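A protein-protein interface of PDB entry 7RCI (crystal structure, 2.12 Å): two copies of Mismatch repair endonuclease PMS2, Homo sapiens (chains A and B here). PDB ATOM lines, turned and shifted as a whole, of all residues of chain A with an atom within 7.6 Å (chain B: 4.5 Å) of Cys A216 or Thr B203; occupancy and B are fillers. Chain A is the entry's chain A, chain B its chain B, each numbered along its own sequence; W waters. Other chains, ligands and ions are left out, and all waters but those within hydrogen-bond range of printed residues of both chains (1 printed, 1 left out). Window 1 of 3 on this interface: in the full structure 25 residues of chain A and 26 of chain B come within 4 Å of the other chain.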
ATOM      1  N   ASP A  55     -33.975  19.389   7.938  1.00  0.00           N
ATOM      2  CA  ASP A  55     -33.013  18.746   8.822  1.00  0.00           C
ATOM      3  C   ASP A  55     -33.280  17.250   8.837  1.00  0.00           C
ATOM      4  O   ASP A  55     -34.413  16.820   9.081  1.00  0.00           O
ATOM      5  CB  ASP A  55     -33.104  19.319  10.239  1.00  0.00           C
ATOM      6  CG  ASP A  55     -32.907  20.819  10.272  1.00  0.00           C
ATOM      7  OD1 ASP A  55     -31.944  21.310   9.645  1.00  0.00           O
ATOM      8  OD2 ASP A  55     -33.719  21.510  10.923  1.00  0.00           O
ATOM      9  N   LEU A 188     -28.479  12.278  -1.274  1.00  0.00           N
ATOM     10  CA  LEU A 188     -28.542  13.435  -0.390  1.00  0.00           C
ATOM     11  C   LEU A 188     -27.616  14.539  -0.881  1.00  0.00           C
ATOM     12  O   LEU A 188     -27.984  15.719  -0.862  1.00  0.00           O
ATOM     13  CB  LEU A 188     -28.190  13.011   1.035  1.00  0.00           C
ATOM     14  CG  LEU A 188     -28.231  14.061   2.140  1.00  0.00           C
ATOM     15  CD1 LEU A 188     -29.646  14.581   2.318  1.00  0.00           C
ATOM     16  CD2 LEU A 188     -27.715  13.453   3.430  1.00  0.00           C
ATOM     17  N   HIS A 189     -26.415  14.173  -1.340  1.00  0.00           N
ATOM     18  CA  HIS A 189     -25.505  15.163  -1.905  1.00  0.00           C
ATOM     19  C   HIS A 189     -26.078  15.784  -3.172  1.00  0.00           C
ATOM     20  O   HIS A 189     -25.778  16.941  -3.485  1.00  0.00           O
ATOM     21  CB  HIS A 189     -24.152  14.518  -2.214  1.00  0.00           C
ATOM     22  CG  HIS A 189     -23.319  14.235  -1.004  1.00  0.00           C
ATOM     23  ND1 HIS A 189     -22.063  13.674  -1.084  1.00  0.00           N
ATOM     24  CD2 HIS A 189     -23.556  14.438   0.313  1.00  0.00           C
ATOM     25  CE1 HIS A 189     -21.563  13.539   0.131  1.00  0.00           C
ATOM     26  NE2 HIS A 189     -22.448  13.999   0.997  1.00  0.00           N
ATOM     27  N   CYS A 192     -28.624  18.483  -2.202  1.00  0.00           N
ATOM     28  CA  CYS A 192     -27.945  19.627  -1.600  1.00  0.00           C
ATOM     29  C   CYS A 192     -27.388  20.566  -2.661  1.00  0.00           C
ATOM     30  O   CYS A 192     -27.431  21.792  -2.499  1.00  0.00           O
ATOM     31  CB  CYS A 192     -26.820  19.149  -0.682  1.00  0.00           C
ATOM     32  SG  CYS A 192     -27.355  18.351   0.837  1.00  0.00           S
ATOM     33  N   ILE A 198     -31.813  26.859   0.014  1.00  0.00           N
ATOM     34  CA  ILE A 198     -32.424  25.995   1.018  1.00  0.00           C
ATOM     35  C   ILE A 198     -31.320  25.410   1.886  1.00  0.00           C
ATOM     36  O   ILE A 198     -30.334  24.875   1.366  1.00  0.00           O
ATOM     37  CB  ILE A 198     -33.266  24.872   0.379  1.00  0.00           C
ATOM     38  CG1 ILE A 198     -34.341  25.462  -0.539  1.00  0.00           C
ATOM     39  CG2 ILE A 198     -33.902  23.999   1.450  1.00  0.00           C
ATOM     40  CD1 ILE A 198     -35.241  24.422  -1.176  1.00  0.00           C
ATOM     41  N   ARG A 199     -31.478  25.522   3.205  1.00  0.00           N
ATOM     42  CA  ARG A 199     -30.506  24.998   4.162  1.00  0.00           C
ATOM     43  C   ARG A 199     -30.822  23.535   4.443  1.00  0.00           C
ATOM     44  O   ARG A 199     -31.817  23.222   5.104  1.00  0.00           O
ATOM     45  CB  ARG A 199     -30.521  25.818   5.450  1.00  0.00           C
ATOM     46  CG  ARG A 199     -29.996  27.229   5.284  1.00  0.00           C
ATOM     47  CD  ARG A 199     -29.970  27.976   6.603  1.00  0.00           C
ATOM     48  NE  ARG A 199     -29.347  29.285   6.456  1.00  0.00           N
ATOM     49  CZ  ARG A 199     -30.003  30.397   6.156  1.00  0.00           C
ATOM     50  NH1 ARG A 199     -31.314  30.400   5.979  1.00  0.00           N
ATOM     51  NH2 ARG A 199     -29.325  31.535   6.025  1.00  0.00           N
ATOM     52  N   VAL A 200     -29.974  22.642   3.942  1.00  0.00           N
ATOM     53  CA  VAL A 200     -30.121  21.203   4.126  1.00  0.00           C
ATOM     54  C   VAL A 200     -28.952  20.705   4.962  1.00  0.00           C
ATOM     55  O   VAL A 200     -27.788  20.905   4.594  1.00  0.00           O
ATOM     56  CB  VAL A 200     -30.183  20.461   2.783  1.00  0.00           C
ATOM     57  CG1 VAL A 200     -30.458  18.983   3.007  1.00  0.00           C
ATOM     58  CG2 VAL A 200     -31.237  21.080   1.884  1.00  0.00           C
ATOM     59  N   SER A 201     -29.257  20.042   6.073  1.00  0.00           N
ATOM     60  CA  SER A 201     -28.234  19.516   6.961  1.00  0.00           C
ATOM     61  C   SER A 201     -28.583  18.083   7.334  1.00  0.00           C
ATOM     62  O   SER A 201     -29.745  17.674   7.286  1.00  0.00           O
ATOM     63  CB  SER A 201     -28.093  20.382   8.223  1.00  0.00           C
ATOM     64  OG  SER A 201     -29.178  20.169   9.109  1.00  0.00           O
ATOM     65  N   CYS A 202     -27.559  17.320   7.714  1.00  0.00           N
ATOM     66  CA  CYS A 202     -27.749  15.917   8.052  1.00  0.00           C
ATOM     67  C   CYS A 202     -26.721  15.509   9.098  1.00  0.00           C
ATOM     68  O   CYS A 202     -25.548  15.884   9.005  1.00  0.00           O
ATOM     69  CB  CYS A 202     -27.628  15.029   6.810  1.00  0.00           C
ATOM     70  SG  CYS A 202     -27.845  13.275   7.135  1.00  0.00           S
ATOM     71  N   PRO A 213     -21.320  14.746  11.790  1.00  0.00           N
ATOM     72  CA  PRO A 213     -21.739  15.526  10.618  1.00  0.00           C
ATOM     73  C   PRO A 213     -21.704  14.681   9.356  1.00  0.00           C
ATOM     74  O   PRO A 213     -20.830  13.829   9.184  1.00  0.00           O
ATOM     75  CB  PRO A 213     -20.709  16.661  10.557  1.00  0.00           C
ATOM     76  CG  PRO A 213     -20.109  16.722  11.922  1.00  0.00           C
ATOM     77  CD  PRO A 213     -20.134  15.320  12.446  1.00  0.00           C
ATOM     78  N   VAL A 214     -22.669  14.920   8.471  1.00  0.00           N
ATOM     79  CA  VAL A 214     -22.732  14.191   7.210  1.00  0.00           C
ATOM     80  C   VAL A 214     -22.618  15.162   6.043  1.00  0.00           C
ATOM     81  O   VAL A 214     -21.705  15.057   5.215  1.00  0.00           O
ATOM     82  CB  VAL A 214     -24.025  13.364   7.110  1.00  0.00           C
ATOM     83  CG1 VAL A 214     -24.141  12.723   5.735  1.00  0.00           C
ATOM     84  CG2 VAL A 214     -24.052  12.307   8.202  1.00  0.00           C
ATOM     85  N   VAL A 215     -23.553  16.106   5.963  1.00  0.00           N
ATOM     86  CA  VAL A 215     -23.548  17.113   4.911  1.00  0.00           C
ATOM     87  C   VAL A 215     -24.302  18.324   5.431  1.00  0.00           C
ATOM     88  O   VAL A 215     -25.171  18.204   6.299  1.00  0.00           O
ATOM     89  CB  VAL A 215     -24.162  16.560   3.599  1.00  0.00           C
ATOM     90  CG1 VAL A 215     -25.666  16.419   3.730  1.00  0.00           C
ATOM     91  CG2 VAL A 215     -23.797  17.448   2.418  1.00  0.00           C
ATOM     92  N   CYS A 216     -23.960  19.499   4.907  1.00  0.00           N
ATOM     93  CA  CYS A 216     -24.614  20.724   5.348  1.00  0.00           C
ATOM     94  C   CYS A 216     -24.386  21.824   4.326  1.00  0.00           C
ATOM     95  O   CYS A 216     -23.241  22.096   3.951  1.00  0.00           O
ATOM     96  CB  CYS A 216     -24.091  21.160   6.716  1.00  0.00           C
ATOM     97  SG  CYS A 216     -24.956  22.581   7.376  1.00  0.00           S
ATOM     98  N   THR A 217     -25.471  22.449   3.880  1.00  0.00           N
ATOM     99  CA  THR A 217     -25.422  23.632   3.035  1.00  0.00           C
ATOM    100  C   THR A 217     -25.820  24.867   3.836  1.00  0.00           C
ATOM    101  O   THR A 217     -26.504  24.778   4.861  1.00  0.00           O
ATOM    102  CB  THR A 217     -26.338  23.483   1.816  1.00  0.00           C
ATOM    103  OG1 THR A 217     -27.679  23.224   2.249  1.00  0.00           O
ATOM    104  CG2 THR A 217     -25.864  22.343   0.930  1.00  0.00           C
ATOM    105  N   GLY A 218     -25.389  26.026   3.347  1.00  0.00           N
ATOM    106  CA  GLY A 218     -25.610  27.292   4.016  1.00  0.00           C
ATOM    107  C   GLY A 218     -26.779  28.118   3.521  1.00  0.00           C
ATOM    108  O   GLY A 218     -26.927  29.267   3.956  1.00  0.00           O
ATOM    109  N   GLY A 219     -27.618  27.582   2.639  1.00  0.00           N
ATOM    110  CA  GLY A 219     -28.700  28.364   2.073  1.00  0.00           C
ATOM    111  C   GLY A 219     -28.270  29.336   0.999  1.00  0.00           C
ATOM    112  O   GLY A 219     -28.879  30.401   0.853  1.00  0.00           O
ATOM    113  N   GLU A 225     -21.813  27.658  -4.895  1.00  0.00           N
ATOM    114  CA  GLU A 225     -21.636  27.786  -3.455  1.00  0.00           C
ATOM    115  C   GLU A 225     -22.096  26.534  -2.716  1.00  0.00           C
ATOM    116  O   GLU A 225     -21.511  26.173  -1.689  1.00  0.00           O
ATOM    117  CB  GLU A 225     -22.390  29.020  -2.964  1.00  0.00           C
ATOM    118  CG  GLU A 225     -21.652  30.335  -3.173  1.00  0.00           C
ATOM    119  CD  GLU A 225     -22.427  31.531  -2.650  1.00  0.00           C
ATOM    120  OE1 GLU A 225     -23.643  31.627  -2.928  1.00  0.00           O
ATOM    121  OE2 GLU A 225     -21.822  32.378  -1.961  1.00  0.00           O
ATOM    122  N   ASN A 226     -23.141  25.865  -3.216  1.00  0.00           N
ATOM    123  CA  ASN A 226     -23.581  24.612  -2.609  1.00  0.00           C
ATOM    124  C   ASN A 226     -22.536  23.514  -2.750  1.00  0.00           C
ATOM    125  O   ASN A 226     -22.406  22.668  -1.858  1.00  0.00           O
ATOM    126  CB  ASN A 226     -24.908  24.160  -3.220  1.00  0.00           C
ATOM    127  CG  ASN A 226     -26.092  24.957  -2.708  1.00  0.00           C
ATOM    128  OD1 ASN A 226     -26.005  25.632  -1.682  1.00  0.00           O
ATOM    129  ND2 ASN A 226     -27.209  24.878  -3.419  1.00  0.00           N
ATOM    130  N   GLY A 228     -19.344  23.986  -2.645  1.00  0.00           N
ATOM    131  CA  GLY A 228     -18.363  24.276  -1.613  1.00  0.00           C
ATOM    132  C   GLY A 228     -18.796  23.885  -0.214  1.00  0.00           C
ATOM    133  O   GLY A 228     -17.941  23.693   0.656  1.00  0.00           O
ATOM    134  N   SER A 229     -20.104  23.788   0.030  1.00  0.00           N
ATOM    135  CA  SER A 229     -20.588  23.333   1.329  1.00  0.00           C
ATOM    136  C   SER A 229     -20.599  21.812   1.436  1.00  0.00           C
ATOM    137  O   SER A 229     -20.414  21.272   2.533  1.00  0.00           O
ATOM    138  CB  SER A 229     -21.990  23.879   1.590  1.00  0.00           C
ATOM    139  OG  SER A 229     -21.995  25.293   1.601  1.00  0.00           O
ATOM    140  N   VAL A 230     -20.809  21.113   0.320  1.00  0.00           N
ATOM    141  CA  VAL A 230     -20.897  19.657   0.351  1.00  0.00           C
ATOM    142  C   VAL A 230     -19.512  19.025   0.297  1.00  0.00           C
ATOM    143  O   VAL A 230     -19.232  18.057   1.012  1.00  0.00           O
ATOM    144  CB  VAL A 230     -21.792  19.158  -0.798  1.00  0.00           C
ATOM    145  CG1 VAL A 230     -21.812  17.638  -0.842  1.00  0.00           C
ATOM    146  CG2 VAL A 230     -23.198  19.708  -0.651  1.00  0.00           C
ATOM    147  N   PHE A 231     -18.627  19.552  -0.551  1.00  0.00           N
ATOM    148  CA  PHE A 231     -17.318  18.954  -0.757  1.00  0.00           C
ATOM    149  C   PHE A 231     -16.153  19.858  -0.373  1.00  0.00           C
ATOM    150  O   PHE A 231     -15.018  19.372  -0.314  1.00  0.00           O
ATOM    151  CB  PHE A 231     -17.160  18.510  -2.222  1.00  0.00           C
ATOM    152  CG  PHE A 231     -18.228  17.551  -2.684  1.00  0.00           C
ATOM    153  CD1 PHE A 231     -18.243  16.239  -2.232  1.00  0.00           C
ATOM    154  CD2 PHE A 231     -19.213  17.959  -3.567  1.00  0.00           C
ATOM    155  CE1 PHE A 231     -19.221  15.355  -2.653  1.00  0.00           C
ATOM    156  CE2 PHE A 231     -20.193  17.078  -3.993  1.00  0.00           C
ATOM    157  CZ  PHE A 231     -20.197  15.775  -3.535  1.00  0.00           C
ATOM    158  N   LEU B  56     -27.621  30.029  12.702  1.00  0.00           N
ATOM    159  CA  LEU B  56     -26.345  30.683  12.972  1.00  0.00           C
ATOM    160  C   LEU B  56     -25.259  30.046  12.114  1.00  0.00           C
ATOM    161  O   LEU B  56     -24.986  28.850  12.244  1.00  0.00           O
ATOM    162  CB  LEU B  56     -25.984  30.579  14.453  1.00  0.00           C
ATOM    163  CG  LEU B  56     -24.578  31.031  14.855  1.00  0.00           C
ATOM    164  CD1 LEU B  56     -24.350  32.496  14.526  1.00  0.00           C
ATOM    165  CD2 LEU B  56     -24.350  30.767  16.331  1.00  0.00           C
ATOM    166  N   LYS B  57     -24.629  30.848  11.261  1.00  0.00           N
ATOM    167  CA  LYS B  57     -23.602  30.377  10.341  1.00  0.00           C
ATOM    168  C   LYS B  57     -22.256  30.971  10.731  1.00  0.00           C
ATOM    169  O   LYS B  57     -22.145  32.183  10.941  1.00  0.00           O
ATOM    170  CB  LYS B  57     -23.943  30.749   8.896  1.00  0.00           C
ATOM    171  CG  LYS B  57     -22.964  30.200   7.872  1.00  0.00           C
ATOM    172  CD  LYS B  57     -23.282  30.701   6.476  1.00  0.00           C
ATOM    173  CE  LYS B  57     -24.666  30.267   6.039  1.00  0.00           C
ATOM    174  NZ  LYS B  57     -25.023  30.841   4.714  1.00  0.00           N
ATOM    175  N   LEU B  58     -21.238  30.119  10.814  1.00  0.00           N
ATOM    176  CA  LEU B  58     -19.909  30.520  11.247  1.00  0.00           C
ATOM    177  C   LEU B  58     -18.872  30.088  10.222  1.00  0.00           C
ATOM    178  O   LEU B  58     -19.069  29.120   9.485  1.00  0.00           O
ATOM    179  CB  LEU B  58     -19.547  29.907  12.601  1.00  0.00           C
ATOM    180  CG  LEU B  58     -20.498  30.160  13.766  1.00  0.00           C
ATOM    181  CD1 LEU B  58     -20.212  29.165  14.872  1.00  0.00           C
ATOM    182  CD2 LEU B  58     -20.342  31.581  14.259  1.00  0.00           C
ATOM    183  N   CYS B 202     -27.076  25.785  14.329  1.00  0.00           N
ATOM    184  CA  CYS B 202     -25.759  26.381  14.155  1.00  0.00           C
ATOM    185  C   CYS B 202     -24.905  25.485  13.275  1.00  0.00           C
ATOM    186  O   CYS B 202     -24.933  24.259  13.412  1.00  0.00           O
ATOM    187  CB  CYS B 202     -25.055  26.599  15.497  1.00  0.00           C
ATOM    188  SG  CYS B 202     -23.391  27.289  15.342  1.00  0.00           S
ATOM    189  N   THR B 203     -24.153  26.105  12.369  1.00  0.00           N
ATOM    190  CA  THR B 203     -23.222  25.392  11.511  1.00  0.00           C
ATOM    191  C   THR B 203     -21.884  26.117  11.519  1.00  0.00           C
ATOM    192  O   THR B 203     -21.803  27.316  11.797  1.00  0.00           O
ATOM    193  CB  THR B 203     -23.740  25.284  10.072  1.00  0.00           C
ATOM    194  OG1 THR B 203     -23.753  26.583   9.472  1.00  0.00           O
ATOM    195  CG2 THR B 203     -25.154  24.725  10.061  1.00  0.00           C
ATOM    196  N   ASN B 204     -20.826  25.372  11.215  1.00  0.00           N
ATOM    197  CA  ASN B 204     -19.487  25.934  11.166  1.00  0.00           C
ATOM    198  C   ASN B 204     -18.711  25.305  10.017  1.00  0.00           C
ATOM    199  O   ASN B 204     -18.863  24.113   9.739  1.00  0.00           O
ATOM    200  CB  ASN B 204     -18.763  25.720  12.503  1.00  0.00           C
ATOM    201  CG  ASN B 204     -17.467  26.483  12.592  1.00  0.00           C
ATOM    202  OD1 ASN B 204     -17.298  27.518  11.950  1.00  0.00           O
ATOM    203  ND2 ASN B 204     -16.543  25.986  13.402  1.00  0.00           N
ATOM    204  N   ARG B 211     -18.987  22.455   5.051  1.00  0.00           N
ATOM    205  CA  ARG B 211     -19.804  22.949   6.149  1.00  0.00           C
ATOM    206  C   ARG B 211     -20.328  21.778   6.974  1.00  0.00           C
ATOM    207  O   ARG B 211     -20.861  20.811   6.425  1.00  0.00           O
ATOM    208  CB  ARG B 211     -20.958  23.789   5.607  1.00  0.00           C
ATOM    209  CG  ARG B 211     -21.889  24.311   6.679  1.00  0.00           C
ATOM    210  CD  ARG B 211     -22.587  25.578   6.228  1.00  0.00           C
ATOM    211  NE  ARG B 211     -21.634  26.635   5.916  1.00  0.00           N
ATOM    212  CZ  ARG B 211     -21.037  27.397   6.823  1.00  0.00           C
ATOM    213  NH1 ARG B 211     -21.272  27.246   8.116  1.00  0.00           N
ATOM    214  NH2 ARG B 211     -20.179  28.330   6.421  1.00  0.00           N
ATOM    215  N   GLN B 212     -20.178  21.865   8.295  1.00  0.00           N
ATOM    216  CA  GLN B 212     -20.584  20.777   9.170  1.00  0.00           C
ATOM    217  C   GLN B 212     -21.599  21.240  10.208  1.00  0.00           C
ATOM    218  O   GLN B 212     -21.436  22.312  10.802  1.00  0.00           O
ATOM    219  CB  GLN B 212     -19.374  20.138   9.868  1.00  0.00           C
ATOM    220  CG  GLN B 212     -18.448  19.425   8.900  1.00  0.00           C
ATOM    221  CD  GLN B 212     -17.281  18.755   9.588  1.00  0.00           C
ATOM    222  OE1 GLN B 212     -17.110  18.868  10.801  1.00  0.00           O
ATOM    223  NE2 GLN B 212     -16.446  18.077   8.808  1.00  0.00           N
ATOM    224  N   PRO B 213     -22.654  20.463  10.438  1.00  0.00           N
ATOM    225  CA  PRO B 213     -23.632  20.826  11.469  1.00  0.00           C
ATOM    226  C   PRO B 213     -23.011  20.798  12.856  1.00  0.00           C
ATOM    227  O   PRO B 213     -22.117  20.001  13.148  1.00  0.00           O
ATOM    228  CB  PRO B 213     -24.718  19.753  11.328  1.00  0.00           C
ATOM    229  CG  PRO B 213     -24.530  19.183   9.959  1.00  0.00           C
ATOM    230  CD  PRO B 213     -23.066  19.277   9.672  1.00  0.00           C
ATOM    231  N   VAL B 214     -23.498  21.691  13.714  1.00  0.00           N
ATOM    232  CA  VAL B 214     -22.995  21.806  15.077  1.00  0.00           C
ATOM    233  C   VAL B 214     -24.099  21.445  16.063  1.00  0.00           C
ATOM    234  O   VAL B 214     -23.930  20.547  16.897  1.00  0.00           O
ATOM    235  CB  VAL B 214     -22.447  23.218  15.351  1.00  0.00           C
ATOM    236  CG1 VAL B 214     -22.062  23.360  16.808  1.00  0.00           C
ATOM    237  CG2 VAL B 214     -21.249  23.501  14.458  1.00  0.00           C
HETATM  238  O   HOH W   1     -21.411  19.735   4.166  1.00  0.00           O
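The backbone carbonyl oxygen of Gly A218 lies within hydrogen-bond range of the side-chain amino group of Lys B57. The backbone carbonyl oxygen (O) of Ser A229 is in hydrogen-bond range of the backbone NH (N) of Arg B211, at 3.1 Å.
Among the printed residues, merely in contact across the chains: Cys A202 with Pro B213, Pro A213 with Gln B212, Pro A213 with Pro B213, Val A215 with Pro B213, Cys A216 with Thr B203, Cys A216 with Arg B211 and Cys A216 with Pro B213.
Of chain B, only Thr B203 (3.4 Å), Arg B211 (3.3 Å) and Pro B213 (3.7 Å) come within 4 Å of Cys A216. No residue of chain A comes within 4 Å of Cys B202. Of chain A, only Cys A216 (3.4 Å) comes within 4 Å of Thr B203. Printed residues of chain A within 4 Å of Arg B211: Cys A216 (3.3 Å) and Ser A229 (3.1 Å). Printed residues of chain A within 4 Å of Gln B212: Pro A213. The nearest residue of chain B that does not touch Cys A216 is Gln B212 (4.3 Å). The nearest residue of chain A that does not touch Thr B203 is Thr A217 (5.4 Å).
The backbone carbonyl oxygen (O) of Cys A202 sits at hydrogen-bond distance from the backbone NH (N) of Val A214, 3.1 Å away. N of Cys A202 lies within hydrogen-bond range of O of Val A215 (2.9 Å). N of Thr B203 sits at hydrogen-bond distance from O of Leu B56 (2.9 Å). The backbone NH (N) of Leu B58 sits at hydrogen-bond distance from the backbone carbonyl oxygen (O) of Thr B203 (3.0 Å). The backbone carbonyl oxygen (O) of Leu B58 is in hydrogen-bond range of the guanidinium group (NH1) of Arg B211 (3.2 Å). N of Gln B212 sits at hydrogen-bond distance from O of Asn B204 (3.0 Å).
Cys A202 touches Pro B213, but with the chains exchanged Pro A213 does not touch Cys B202 (9.1 Å). Pro B213 touches its own counterpart, Pro A213. Positions printed for both chains: 202, 213 and 214.
Water W1 lies within hydrogen-bond range of the backbone carbonyl oxygen (O) of Ser A229, the backbone carbonyl oxygen (O) of Arg B211 and the backbone NH (N) of Cys A216.
Of the 22 printed residues of chain A, 6 touch a printed residue of chain B. Hydrophobic or aromatic side chains of chain A within 4 Å of the printed part of chain B: Pro A213. Hydrophobic or aromatic side chains of chain B that line the printed part of chain A: Pro B213.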
